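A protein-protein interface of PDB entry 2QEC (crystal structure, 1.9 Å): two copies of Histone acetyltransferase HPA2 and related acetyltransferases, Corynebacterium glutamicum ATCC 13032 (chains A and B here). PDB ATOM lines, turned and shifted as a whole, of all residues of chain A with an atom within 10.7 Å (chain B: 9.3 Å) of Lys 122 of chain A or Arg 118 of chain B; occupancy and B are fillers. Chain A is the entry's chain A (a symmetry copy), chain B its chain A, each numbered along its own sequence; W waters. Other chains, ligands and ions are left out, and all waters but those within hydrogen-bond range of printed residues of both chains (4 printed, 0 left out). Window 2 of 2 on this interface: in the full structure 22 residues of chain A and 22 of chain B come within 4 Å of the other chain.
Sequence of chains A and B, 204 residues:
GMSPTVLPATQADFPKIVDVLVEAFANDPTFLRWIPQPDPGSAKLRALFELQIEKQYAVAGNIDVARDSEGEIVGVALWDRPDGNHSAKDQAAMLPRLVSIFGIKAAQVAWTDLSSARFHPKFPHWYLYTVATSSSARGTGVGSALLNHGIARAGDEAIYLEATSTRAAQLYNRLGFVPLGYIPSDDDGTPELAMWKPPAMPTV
Phe 119 of chain A touches Lys 122 of chain B, and with the chains exchanged Lys 122 of chain A touches Phe 119 of chain B.
Phe 123 of chain A touches Leu 180 of chain B, and with the chains exchanged Leu 180 of chain A touches Phe 123 of chain B.
10 positions are printed for both chains.
Of the 14 pairs that touch across the chains among the printed residues, 8 have their exchanged pair printed and touching as well.
Printed residues of chain A that touch a printed residue of chain B: Arg 118, Phe 119, Lys 122, Phe 123, Leu 180, Trp 196 and Pro 199.
Hydrophobic or aromatic side chains of chain A within 4 Å of the printed part of chain B: Phe 119, Phe 123, Leu 180, Trp 196 and Pro 199.
Of the 18 printed residues of chain B, 9 touch a printed residue of chain A.
Hydrophobic or aromatic side chains of chain B within 4 Å of the printed part of chain A: Phe 119, Phe 123, Leu 180, Ile 183 and Ala 194.
Lys 122 of chain A touches two residues of chain B.
Of the printed residues of chain A, Arg 118 of chain B touches Lys 122.
Phe 123 of chain A touches six residues of chain B.
No residue of chain A comes within 4 Å of Ala 117 of chain B.
Of chain A, only Lys 122 and Phe 123 come within 4 Å of Phe 119 of chain B.
No residue of chain A comes within 4 Å of His 120 of chain B.
Of the printed residues of chain A, Tyr 182 of chain B touches Phe 123 (3.7 Å).
Of the printed residues of chain A, Leu 180 of chain B touches Phe 123 (3.6 Å), Trp 196 (3.4 Å) and Pro 199 (3.9 Å).
Of the printed residues of chain A, Ala 194 of chain B touches Phe 123 (3.3 Å).
Trp 126 of chain A touches none of the printed residues of chain B.
The nearest residue of chain A that does not touch Arg 118 of chain B is Phe 123 of chain A (6.7 Å).
The nearest printed residue of chain A that does not touch Leu 180 of chain B is Leu 180 of chain A (4.5 Å).
A ring nitrogen (ND1) of His 125 of chain B is in hydrogen-bond range of the backbone carbonyl oxygen of Phe 123 of chain B, at 2.8 Å.
N of Leu 180 of chain B lies within hydrogen-bond range of O of Ala 194 of chain B, at 2.9 Å.
O of Phe 123 of chain A is in hydrogen-bond range of ND1 of His 125 of chain A (2.8 Å).
Among the printed residues, merely in contact across the chains: Phe 123 of chain A with Ala 194 of chain B, Trp 196 of chain A with Leu 180 of chain B, Phe 123 of chain A with Gly 181 of chain B, Phe 123 of chain A with Phe 119 of chain B, Phe 119 of chain A with Phe 123 of chain B, Leu 180 of chain A with Phe 123 of chain B, Phe 123 of chain A with Leu 180 of chain B, Phe 123 of chain A with Tyr 182 of chain B, Arg 118 of chain A with Lys 122 of chain B, Lys 122 of chain A with Arg 118 of chain B, Phe 119 of chain A with Lys 122 of chain B, Lys 122 of chain A with Phe 119 of chain B, Phe 123 of chain A with Ile 183 of chain B and Pro 199 of chain A with Leu 180 of chain B.
Water W2 lies within hydrogen-bond range of O of Lys 122 of chain A (2.7 Å) and O of Tyr 182 of chain B (3.3 Å).
Water W1 lies within hydrogen-bond range of the backbone carbonyl oxygen of Leu 180 of chain B (2.8 Å) and the backbone carbonyl oxygen of Pro 124 of chain A (2.9 Å).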
ATOM      1  N   PRO A  82      -4.499 -12.033  29.023  1.00  0.00           N
ATOM      2  CA  PRO A  82      -5.275 -11.867  27.809  1.00  0.00           C
ATOM      3  C   PRO A  82      -4.600 -11.046  26.685  1.00  0.00           C
ATOM      4  O   PRO A  82      -3.867 -10.092  26.952  1.00  0.00           O
ATOM      5  CB  PRO A  82      -6.572 -11.167  28.282  1.00  0.00           C
ATOM      6  CG  PRO A  82      -6.643 -11.332  29.689  1.00  0.00           C
ATOM      7  CD  PRO A  82      -5.207 -11.505  30.205  1.00  0.00           C
ATOM      8  N   ASP A  83      -4.870 -11.431  25.439  1.00  0.00           N
ATOM      9  CA  ASP A  83      -4.353 -10.722  24.256  1.00  0.00           C
ATOM     10  C   ASP A  83      -5.180 -11.116  23.020  1.00  0.00           C
ATOM     11  O   ASP A  83      -4.780 -10.873  21.877  1.00  0.00           O
ATOM     12  CB  ASP A  83      -2.858 -11.025  24.023  1.00  0.00           C
ATOM     13  N   ALA A 117      -2.742 -23.712  21.386  1.00  0.00           N
ATOM     14  CA  ALA A 117      -3.514 -22.580  20.882  1.00  0.00           C
ATOM     15  C   ALA A 117      -4.908 -23.001  20.412  1.00  0.00           C
ATOM     16  O   ALA A 117      -5.899 -22.306  20.677  1.00  0.00           O
ATOM     17  CB  ALA A 117      -2.765 -21.935  19.719  1.00  0.00           C
ATOM     18  N   ARG A 118      -4.973 -24.111  19.677  1.00  0.00           N
ATOM     19  CA  ARG A 118      -6.132 -24.371  18.795  1.00  0.00           C
ATOM     20  C   ARG A 118      -7.480 -24.628  19.503  1.00  0.00           C
ATOM     21  O   ARG A 118      -8.573 -24.317  18.961  1.00  0.00           O
ATOM     22  CB  ARG A 118      -5.825 -25.524  17.814  1.00  0.00           C
ATOM     23  N   PHE A 119      -7.418 -25.133  20.725  1.00  0.00           N
ATOM     24  CA  PHE A 119      -8.629 -25.457  21.486  1.00  0.00           C
ATOM     25  C   PHE A 119      -9.046 -24.356  22.458  1.00  0.00           C
ATOM     26  O   PHE A 119     -10.101 -24.454  23.068  1.00  0.00           O
ATOM     27  CB  PHE A 119      -8.405 -26.775  22.216  1.00  0.00           C
ATOM     28  CG  PHE A 119      -8.316 -27.953  21.295  1.00  0.00           C
ATOM     29  CD1 PHE A 119      -9.457 -28.566  20.825  1.00  0.00           C
ATOM     30  CD2 PHE A 119      -7.080 -28.445  20.877  1.00  0.00           C
ATOM     31  CE1 PHE A 119      -9.399 -29.637  19.975  1.00  0.00           C
ATOM     32  CE2 PHE A 119      -7.018 -29.526  20.004  1.00  0.00           C
ATOM     33  CZ  PHE A 119      -8.178 -30.131  19.565  1.00  0.00           C
ATOM     34  N   HIS A 120      -8.245 -23.292  22.574  1.00  0.00           N
ATOM     35  CA  HIS A 120      -8.621 -22.124  23.336  1.00  0.00           C
ATOM     36  C   HIS A 120      -9.758 -21.391  22.634  1.00  0.00           C
ATOM     37  O   HIS A 120      -9.689 -21.094  21.441  1.00  0.00           O
ATOM     38  CB  HIS A 120      -7.485 -21.114  23.504  1.00  0.00           C
ATOM     39  CG  HIS A 120      -6.312 -21.628  24.269  1.00  0.00           C
ATOM     40  ND1 HIS A 120      -5.695 -20.903  25.271  1.00  0.00           N
ATOM     41  CD2 HIS A 120      -5.612 -22.784  24.156  1.00  0.00           C
ATOM     42  CE1 HIS A 120      -4.690 -21.598  25.754  1.00  0.00           C
ATOM     43  NE2 HIS A 120      -4.610 -22.738  25.098  1.00  0.00           N
ATOM     44  N   PRO A 121     -10.791 -21.068  23.376  1.00  0.00           N
ATOM     45  CA  PRO A 121     -11.841 -20.232  22.776  1.00  0.00           C
ATOM     46  C   PRO A 121     -11.300 -18.898  22.208  1.00  0.00           C
ATOM     47  O   PRO A 121     -10.284 -18.377  22.656  1.00  0.00           O
ATOM     48  CB  PRO A 121     -12.853 -20.059  23.923  1.00  0.00           C
ATOM     49  CG  PRO A 121     -12.541 -21.251  24.864  1.00  0.00           C
ATOM     50  CD  PRO A 121     -11.076 -21.412  24.778  1.00  0.00           C
ATOM     51  N   LYS A 122     -11.922 -18.404  21.144  1.00  0.00           N
ATOM     52  CA  LYS A 122     -11.375 -17.249  20.435  1.00  0.00           C
ATOM     53  C   LYS A 122     -11.927 -15.975  21.035  1.00  0.00           C
ATOM     54  O   LYS A 122     -12.551 -15.166  20.360  1.00  0.00           O
ATOM     55  CB  LYS A 122     -11.727 -17.317  18.950  1.00  0.00           C
ATOM     56  CG  LYS A 122     -11.248 -18.595  18.260  1.00  0.00           C
ATOM     57  CD  LYS A 122      -9.722 -18.625  18.124  1.00  0.00           C
ATOM     58  CE  LYS A 122      -9.231 -19.762  17.198  1.00  0.00           C
ATOM     59  NZ  LYS A 122      -7.733 -19.820  17.171  1.00  0.00           N
ATOM     60  N   PHE A 123     -11.712 -15.826  22.320  1.00  0.00           N
ATOM     61  CA  PHE A 123     -12.167 -14.676  23.086  1.00  0.00           C
ATOM     62  C   PHE A 123     -11.077 -14.430  24.114  1.00  0.00           C
ATOM     63  O   PHE A 123     -10.388 -15.367  24.492  1.00  0.00           O
ATOM     64  CB  PHE A 123     -13.471 -15.011  23.805  1.00  0.00           C
ATOM     65  CG  PHE A 123     -14.574 -15.400  22.868  1.00  0.00           C
ATOM     66  CD1 PHE A 123     -15.292 -14.427  22.227  1.00  0.00           C
ATOM     67  CD2 PHE A 123     -14.841 -16.738  22.583  1.00  0.00           C
ATOM     68  CE1 PHE A 123     -16.303 -14.769  21.317  1.00  0.00           C
ATOM     69  CE2 PHE A 123     -15.822 -17.089  21.701  1.00  0.00           C
ATOM     70  CZ  PHE A 123     -16.569 -16.091  21.077  1.00  0.00           C
ATOM     71  N   PRO A 124     -10.912 -13.172  24.561  1.00  0.00           N
ATOM     72  CA  PRO A 124      -9.799 -12.868  25.485  1.00  0.00           C
ATOM     73  C   PRO A 124      -9.911 -13.624  26.778  1.00  0.00           C
ATOM     74  O   PRO A 124     -11.014 -13.791  27.329  1.00  0.00           O
ATOM     75  CB  PRO A 124      -9.927 -11.354  25.722  1.00  0.00           C
ATOM     76  CG  PRO A 124     -10.782 -10.854  24.568  1.00  0.00           C
ATOM     77  CD  PRO A 124     -11.699 -11.972  24.211  1.00  0.00           C
ATOM     78  N   HIS A 125      -8.779 -14.143  27.252  1.00  0.00           N
ATOM     79  CA  HIS A 125      -8.784 -14.902  28.458  1.00  0.00           C
ATOM     80  C   HIS A 125      -7.402 -14.986  29.038  1.00  0.00           C
ATOM     81  O   HIS A 125      -6.407 -14.916  28.304  1.00  0.00           O
ATOM     82  CB  HIS A 125      -9.285 -16.347  28.203  1.00  0.00           C
ATOM     83  CG  HIS A 125      -8.458 -17.123  27.215  1.00  0.00           C
ATOM     84  ND1 HIS A 125      -8.689 -17.048  25.857  1.00  0.00           N
ATOM     85  CD2 HIS A 125      -7.428 -17.994  27.376  1.00  0.00           C
ATOM     86  CE1 HIS A 125      -7.817 -17.823  25.227  1.00  0.00           C
ATOM     87  NE2 HIS A 125      -7.050 -18.419  26.125  1.00  0.00           N
ATOM     88  N   TRP A 126      -7.343 -15.224  30.349  1.00  0.00           N
ATOM     89  CA  TRP A 126      -6.112 -15.695  30.996  1.00  0.00           C
ATOM     90  C   TRP A 126      -5.930 -17.191  30.727  1.00  0.00           C
ATOM     91  O   TRP A 126      -6.892 -17.896  30.550  1.00  0.00           O
ATOM     92  CB  TRP A 126      -6.177 -15.502  32.504  1.00  0.00           C
ATOM     93  CG  TRP A 126      -6.181 -14.076  32.934  1.00  0.00           C
ATOM     94  CD1 TRP A 126      -7.225 -13.181  32.855  1.00  0.00           C
ATOM     95  CD2 TRP A 126      -5.079 -13.366  33.438  1.00  0.00           C
ATOM     96  NE1 TRP A 126      -6.823 -11.950  33.322  1.00  0.00           N
ATOM     97  CE2 TRP A 126      -5.509 -12.055  33.713  1.00  0.00           C
ATOM     98  CE3 TRP A 126      -3.738 -13.737  33.764  1.00  0.00           C
ATOM     99  CZ2 TRP A 126      -4.660 -11.103  34.263  1.00  0.00           C
ATOM    100  CZ3 TRP A 126      -2.915 -12.788  34.289  1.00  0.00           C
ATOM    101  CH2 TRP A 126      -3.375 -11.495  34.549  1.00  0.00           C
ATOM    102  N   ALA A 158     -12.020 -13.748  31.934  1.00  0.00           N
ATOM    103  CA  ALA A 158     -12.101 -15.191  31.713  1.00  0.00           C
ATOM    104  C   ALA A 158     -10.752 -15.900  31.922  1.00  0.00           C
ATOM    105  O   ALA A 158      -9.692 -15.318  31.762  1.00  0.00           O
ATOM    106  CB  ALA A 158     -12.604 -15.442  30.320  1.00  0.00           C
ATOM    107  N   TYR A 160      -8.954 -19.812  30.875  1.00  0.00           N
ATOM    108  CA  TYR A 160      -8.882 -21.155  30.266  1.00  0.00           C
ATOM    109  C   TYR A 160      -7.801 -22.013  30.954  1.00  0.00           C
ATOM    110  O   TYR A 160      -6.764 -21.504  31.337  1.00  0.00           O
ATOM    111  CB  TYR A 160      -8.571 -20.987  28.753  1.00  0.00           C
ATOM    112  CG  TYR A 160      -8.397 -22.268  27.954  1.00  0.00           C
ATOM    113  CD1 TYR A 160      -9.470 -22.967  27.493  1.00  0.00           C
ATOM    114  CD2 TYR A 160      -7.125 -22.799  27.719  1.00  0.00           C
ATOM    115  CE1 TYR A 160      -9.311 -24.172  26.766  1.00  0.00           C
ATOM    116  CE2 TYR A 160      -6.951 -23.997  27.015  1.00  0.00           C
ATOM    117  CZ  TYR A 160      -8.079 -24.664  26.516  1.00  0.00           C
ATOM    118  OH  TYR A 160      -7.950 -25.844  25.807  1.00  0.00           O
ATOM    119  N   LEU A 180     -15.558 -27.330  28.929  1.00  0.00           N
ATOM    120  CA  LEU A 180     -15.722 -27.144  27.493  1.00  0.00           C
ATOM    121  C   LEU A 180     -15.781 -28.536  26.835  1.00  0.00           C
ATOM    122  O   LEU A 180     -16.730 -28.866  26.160  1.00  0.00           O
ATOM    123  CB  LEU A 180     -14.556 -26.327  26.955  1.00  0.00           C
ATOM    124  CG  LEU A 180     -14.480 -24.850  27.379  1.00  0.00           C
ATOM    125  CD1 LEU A 180     -13.158 -24.231  26.896  1.00  0.00           C
ATOM    126  CD2 LEU A 180     -15.610 -24.055  26.742  1.00  0.00           C
ATOM    127  N   TRP A 196     -13.352 -23.514  31.344  1.00  0.00           N
ATOM    128  CA  TRP A 196     -13.507 -22.091  31.197  1.00  0.00           C
ATOM    129  C   TRP A 196     -14.115 -21.505  32.447  1.00  0.00           C
ATOM    130  O   TRP A 196     -15.256 -21.864  32.799  1.00  0.00           O
ATOM    131  CB  TRP A 196     -14.495 -21.870  30.049  1.00  0.00           C
ATOM    132  CG  TRP A 196     -14.761 -20.462  29.573  1.00  0.00           C
ATOM    133  CD1 TRP A 196     -15.917 -19.763  29.709  1.00  0.00           C
ATOM    134  CD2 TRP A 196     -13.882 -19.638  28.808  1.00  0.00           C
ATOM    135  NE1 TRP A 196     -15.811 -18.543  29.090  1.00  0.00           N
ATOM    136  CE2 TRP A 196     -14.570 -18.437  28.529  1.00  0.00           C
ATOM    137  CE3 TRP A 196     -12.577 -19.793  28.334  1.00  0.00           C
ATOM    138  CZ2 TRP A 196     -13.997 -17.406  27.793  1.00  0.00           C
ATOM    139  CZ3 TRP A 196     -12.000 -18.758  27.607  1.00  0.00           C
ATOM    140  CH2 TRP A 196     -12.708 -17.587  27.336  1.00  0.00           C
ATOM    141  N   PRO A 199     -16.164 -14.814  31.930  1.00  0.00           N
ATOM    142  CA  PRO A 199     -16.053 -13.427  32.319  1.00  0.00           C
ATOM    143  C   PRO A 199     -17.353 -13.005  32.976  1.00  0.00           C
ATOM    144  O   PRO A 199     -18.343 -13.723  32.899  1.00  0.00           O
ATOM    145  CB  PRO A 199     -15.795 -12.722  30.996  1.00  0.00           C
ATOM    146  CG  PRO A 199     -16.531 -13.541  29.994  1.00  0.00           C
ATOM    147  CD  PRO A 199     -16.323 -14.964  30.477  1.00  0.00           C
ATOM    148  N   ALA B 107     -20.494 -18.727   3.793  1.00  0.00           N
ATOM    149  CA  ALA B 107     -19.686 -19.637   4.617  1.00  0.00           C
ATOM    150  C   ALA B 107     -18.806 -18.908   5.636  1.00  0.00           C
ATOM    151  O   ALA B 107     -19.284 -18.087   6.419  1.00  0.00           O
ATOM    152  CB  ALA B 107     -18.827 -20.530   3.729  1.00  0.00           C
ATOM    153  N   ALA B 117     -18.744 -20.405  12.007  1.00  0.00           N
ATOM    154  CA  ALA B 117     -17.937 -21.538  12.450  1.00  0.00           C
ATOM    155  C   ALA B 117     -16.838 -21.112  13.426  1.00  0.00           C
ATOM    156  O   ALA B 117     -16.588 -21.793  14.430  1.00  0.00           O
ATOM    157  CB  ALA B 117     -17.298 -22.209  11.237  1.00  0.00           C
ATOM    158  N   ARG B 118     -16.156 -20.013  13.104  1.00  0.00           N
ATOM    159  CA  ARG B 118     -14.816 -19.756  13.675  1.00  0.00           C
ATOM    160  C   ARG B 118     -14.767 -19.475  15.192  1.00  0.00           C
ATOM    161  O   ARG B 118     -13.761 -19.785  15.883  1.00  0.00           O
ATOM    162  CB  ARG B 118     -14.101 -18.622  12.907  1.00  0.00           C
ATOM    163  N   PHE B 119     -15.857 -18.952  15.731  1.00  0.00           N
ATOM    164  CA  PHE B 119     -15.921 -18.603  17.154  1.00  0.00           C
ATOM    165  C   PHE B 119     -16.573 -19.685  18.013  1.00  0.00           C
ATOM    166  O   PHE B 119     -16.585 -19.567  19.229  1.00  0.00           O
ATOM    167  CB  PHE B 119     -16.655 -17.276  17.297  1.00  0.00           C
ATOM    168  CG  PHE B 119     -15.886 -16.114  16.748  1.00  0.00           C
ATOM    169  CD1 PHE B 119     -14.909 -15.498  17.500  1.00  0.00           C
ATOM    170  CD2 PHE B 119     -16.125 -15.641  15.458  1.00  0.00           C
ATOM    171  CE1 PHE B 119     -14.188 -14.441  17.015  1.00  0.00           C
ATOM    172  CE2 PHE B 119     -15.385 -14.574  14.958  1.00  0.00           C
ATOM    173  CZ  PHE B 119     -14.427 -13.966  15.743  1.00  0.00           C
ATOM    174  N   HIS B 120     -17.078 -20.754  17.390  1.00  0.00           N
ATOM    175  CA  HIS B 120     -17.568 -21.906  18.110  1.00  0.00           C
ATOM    176  C   HIS B 120     -16.404 -22.640  18.767  1.00  0.00           C
ATOM    177  O   HIS B 120     -15.402 -22.957  18.126  1.00  0.00           O
ATOM    178  CB  HIS B 120     -18.282 -22.925  17.220  1.00  0.00           C
ATOM    179  CG  HIS B 120     -19.519 -22.409  16.566  1.00  0.00           C
ATOM    180  ND1 HIS B 120     -20.703 -23.124  16.532  1.00  0.00           N
ATOM    181  CD2 HIS B 120     -19.755 -21.262  15.882  1.00  0.00           C
ATOM    182  CE1 HIS B 120     -21.610 -22.431  15.884  1.00  0.00           C
ATOM    183  NE2 HIS B 120     -21.068 -21.302  15.473  1.00  0.00           N
ATOM    184  N   PRO B 121     -16.545 -22.942  20.036  1.00  0.00           N
ATOM    185  CA  PRO B 121     -15.514 -23.777  20.669  1.00  0.00           C
ATOM    186  C   PRO B 121     -15.299 -25.125  19.940  1.00  0.00           C
ATOM    187  O   PRO B 121     -16.193 -25.649  19.284  1.00  0.00           O
ATOM    188  CB  PRO B 121     -16.017 -23.923  22.117  1.00  0.00           C
ATOM    189  CG  PRO B 121     -16.979 -22.719  22.288  1.00  0.00           C
ATOM    190  CD  PRO B 121     -17.623 -22.573  20.968  1.00  0.00           C
ATOM    191  N   LYS B 122     -14.071 -25.630  19.967  1.00  0.00           N
ATOM    192  CA  LYS B 122     -13.733 -26.801  19.161  1.00  0.00           C
ATOM    193  C   LYS B 122     -13.996 -28.060  19.957  1.00  0.00           C
ATOM    194  O   LYS B 122     -13.109 -28.875  20.181  1.00  0.00           O
ATOM    195  CB  LYS B 122     -12.266 -26.754  18.736  1.00  0.00           C
ATOM    196  CG  LYS B 122     -11.889 -25.492  17.960  1.00  0.00           C
ATOM    197  CD  LYS B 122     -12.520 -25.478  16.564  1.00  0.00           C
ATOM    198  CE  LYS B 122     -11.944 -24.361  15.663  1.00  0.00           C
ATOM    199  NZ  LYS B 122     -12.657 -24.318  14.344  1.00  0.00           N
ATOM    200  N   PHE B 123     -15.223 -28.191  20.404  1.00  0.00           N
ATOM    201  CA  PHE B 123     -15.677 -29.324  21.194  1.00  0.00           C
ATOM    202  C   PHE B 123     -17.110 -29.564  20.755  1.00  0.00           C
ATOM    203  O   PHE B 123     -17.769 -28.628  20.325  1.00  0.00           O
ATOM    204  CB  PHE B 123     -15.659 -28.966  22.678  1.00  0.00           C
ATOM    205  CG  PHE B 123     -14.297 -28.581  23.172  1.00  0.00           C
ATOM    206  CD1 PHE B 123     -13.394 -29.557  23.497  1.00  0.00           C
ATOM    207  CD2 PHE B 123     -13.904 -27.245  23.243  1.00  0.00           C
ATOM    208  CE1 PHE B 123     -12.102 -29.221  23.925  1.00  0.00           C
ATOM    209  CE2 PHE B 123     -12.651 -26.900  23.658  1.00  0.00           C
ATOM    210  CZ  PHE B 123     -11.750 -27.901  24.018  1.00  0.00           C
ATOM    211  N   HIS B 125     -20.975 -29.822  20.299  1.00  0.00           N
ATOM    212  CA  HIS B 125     -22.015 -29.044  20.884  1.00  0.00           C
ATOM    213  C   HIS B 125     -23.199 -28.964  19.965  1.00  0.00           C
ATOM    214  O   HIS B 125     -23.049 -29.054  18.739  1.00  0.00           O
ATOM    215  CB  HIS B 125     -21.533 -27.598  21.172  1.00  0.00           C
ATOM    216  CG  HIS B 125     -21.072 -26.846  19.955  1.00  0.00           C
ATOM    217  ND1 HIS B 125     -19.777 -26.941  19.489  1.00  0.00           N
ATOM    218  CD2 HIS B 125     -21.711 -25.982  19.123  1.00  0.00           C
ATOM    219  CE1 HIS B 125     -19.650 -26.184  18.408  1.00  0.00           C
ATOM    220  NE2 HIS B 125     -20.804 -25.581  18.172  1.00  0.00           N
ATOM    221  N   TYR B 127     -25.937 -26.282  18.365  1.00  0.00           N
ATOM    222  CA  TYR B 127     -25.939 -24.851  18.046  1.00  0.00           C
ATOM    223  C   TYR B 127     -27.363 -24.422  17.853  1.00  0.00           C
ATOM    224  O   TYR B 127     -27.996 -24.965  17.001  1.00  0.00           O
ATOM    225  CB  TYR B 127     -25.174 -24.605  16.746  1.00  0.00           C
ATOM    226  CG  TYR B 127     -25.186 -23.204  16.144  1.00  0.00           C
ATOM    227  CD1 TYR B 127     -25.126 -22.066  16.936  1.00  0.00           C
ATOM    228  CD2 TYR B 127     -25.247 -23.027  14.758  1.00  0.00           C
ATOM    229  CE1 TYR B 127     -25.132 -20.817  16.392  1.00  0.00           C
ATOM    230  CE2 TYR B 127     -25.240 -21.782  14.211  1.00  0.00           C
ATOM    231  CZ  TYR B 127     -25.165 -20.682  15.025  1.00  0.00           C
ATOM    232  OH  TYR B 127     -25.180 -19.430  14.480  1.00  0.00           O
ATOM    233  N   TYR B 160     -23.991 -24.094  22.142  1.00  0.00           N
ATOM    234  CA  TYR B 160     -23.483 -22.761  21.758  1.00  0.00           C
ATOM    235  C   TYR B 160     -24.606 -21.903  21.141  1.00  0.00           C
ATOM    236  O   TYR B 160     -25.454 -22.416  20.435  1.00  0.00           O
ATOM    237  CB  TYR B 160     -22.320 -22.957  20.746  1.00  0.00           C
ATOM    238  CG  TYR B 160     -21.697 -21.691  20.181  1.00  0.00           C
ATOM    239  CD1 TYR B 160     -20.762 -20.989  20.879  1.00  0.00           C
ATOM    240  CD2 TYR B 160     -22.113 -21.175  18.950  1.00  0.00           C
ATOM    241  CE1 TYR B 160     -20.196 -19.798  20.364  1.00  0.00           C
ATOM    242  CE2 TYR B 160     -21.575 -19.991  18.434  1.00  0.00           C
ATOM    243  CZ  TYR B 160     -20.579 -19.321  19.160  1.00  0.00           C
ATOM    244  OH  TYR B 160     -20.014 -18.154  18.680  1.00  0.00           O
ATOM    245  N   GLU B 162     -25.251 -17.346  20.044  1.00  0.00           N
ATOM    246  CA  GLU B 162     -24.758 -15.972  19.999  1.00  0.00           C
ATOM    247  C   GLU B 162     -25.889 -15.050  20.305  1.00  0.00           C
ATOM    248  O   GLU B 162     -26.819 -14.955  19.506  1.00  0.00           O
ATOM    249  CB  GLU B 162     -24.189 -15.714  18.623  1.00  0.00           C
ATOM    250  CG  GLU B 162     -22.831 -16.423  18.467  1.00  0.00           C
ATOM    251  CD  GLU B 162     -22.396 -16.635  17.021  1.00  0.00           C
ATOM    252  OE1 GLU B 162     -23.137 -16.219  16.128  1.00  0.00           O
ATOM    253  OE2 GLU B 162     -21.280 -17.175  16.787  1.00  0.00           O
ATOM    254  N   LEU B 180     -18.979 -16.547  26.815  1.00  0.00           N
ATOM    255  CA  LEU B 180     -17.650 -16.754  26.255  1.00  0.00           C
ATOM    256  C   LEU B 180     -17.035 -15.373  25.961  1.00  0.00           C
ATOM    257  O   LEU B 180     -15.978 -15.044  26.451  1.00  0.00           O
ATOM    258  CB  LEU B 180     -17.762 -17.591  24.989  1.00  0.00           C
ATOM    259  CG  LEU B 180     -18.183 -19.061  25.155  1.00  0.00           C
ATOM    260  CD1 LEU B 180     -18.417 -19.700  23.776  1.00  0.00           C
ATOM    261  CD2 LEU B 180     -17.080 -19.856  25.838  1.00  0.00           C
ATOM    262  N   GLY B 181     -17.730 -14.549  25.205  1.00  0.00           N
ATOM    263  CA  GLY B 181     -17.284 -13.164  24.973  1.00  0.00           C
ATOM    264  C   GLY B 181     -17.962 -12.599  23.746  1.00  0.00           C
ATOM    265  O   GLY B 181     -18.807 -13.263  23.149  1.00  0.00           O
ATOM    266  N   TYR B 182     -17.624 -11.362  23.390  1.00  0.00           N
ATOM    267  CA  TYR B 182     -18.246 -10.707  22.236  1.00  0.00           C
ATOM    268  C   TYR B 182     -17.505 -11.052  20.952  1.00  0.00           C
ATOM    269  O   TYR B 182     -16.277 -11.133  20.931  1.00  0.00           O
ATOM    270  CB  TYR B 182     -18.325  -9.188  22.446  1.00  0.00           C
ATOM    271  CG  TYR B 182     -19.355  -8.808  23.472  1.00  0.00           C
ATOM    272  CD1 TYR B 182     -20.691  -8.648  23.108  1.00  0.00           C
ATOM    273  CD2 TYR B 182     -18.994  -8.637  24.813  1.00  0.00           C
ATOM    274  CE1 TYR B 182     -21.640  -8.301  24.062  1.00  0.00           C
ATOM    275  CE2 TYR B 182     -19.936  -8.292  25.768  1.00  0.00           C
ATOM    276  CZ  TYR B 182     -21.236  -8.125  25.395  1.00  0.00           C
ATOM    277  OH  TYR B 182     -22.167  -7.793  26.343  1.00  0.00           O
ATOM    278  N   ILE B 183     -18.268 -11.318  19.898  1.00  0.00           N
ATOM    279  CA  ILE B 183     -17.704 -11.556  18.565  1.00  0.00           C
ATOM    280  C   ILE B 183     -17.594 -10.208  17.843  1.00  0.00           C
ATOM    281  O   ILE B 183     -18.584  -9.467  17.748  1.00  0.00           O
ATOM    282  CB  ILE B 183     -18.597 -12.544  17.753  1.00  0.00           C
ATOM    283  CG1 ILE B 183     -18.565 -13.919  18.394  1.00  0.00           C
ATOM    284  CG2 ILE B 183     -18.193 -12.547  16.255  1.00  0.00           C
ATOM    285  CD1 ILE B 183     -19.644 -14.835  17.945  1.00  0.00           C
ATOM    286  N   PRO B 184     -16.397  -9.880  17.330  1.00  0.00           N
ATOM    287  CA  PRO B 184     -16.264  -8.611  16.609  1.00  0.00           C
ATOM    288  C   PRO B 184     -17.149  -8.561  15.377  1.00  0.00           C
ATOM    289  O   PRO B 184     -17.192  -9.535  14.631  1.00  0.00           O
ATOM    290  CB  PRO B 184     -14.791  -8.576  16.189  1.00  0.00           C
ATOM    291  CG  PRO B 184     -14.110  -9.617  16.973  1.00  0.00           C
ATOM    292  CD  PRO B 184     -15.132 -10.628  17.381  1.00  0.00           C
ATOM    293  N   ALA B 194     -21.304 -14.433  22.415  1.00  0.00           N
ATOM    294  CA  ALA B 194     -21.216 -15.887  22.346  1.00  0.00           C
ATOM    295  C   ALA B 194     -21.412 -16.434  23.734  1.00  0.00           C
ATOM    296  O   ALA B 194     -20.796 -15.934  24.692  1.00  0.00           O
ATOM    297  CB  ALA B 194     -19.801 -16.292  21.853  1.00  0.00           C
HETATM  298  O   HOH W   1     -13.858 -13.375  27.060  1.00  0.00           O
HETATM  299  O   HOH W   2     -13.504 -12.673  20.111  1.00  0.00           O
HETATM  300  O   HOH W   3     -14.086 -20.079  20.410  1.00  0.00           O
HETATM  301  O   HOH W   4     -12.352 -23.947  21.464  1.00  0.00           O
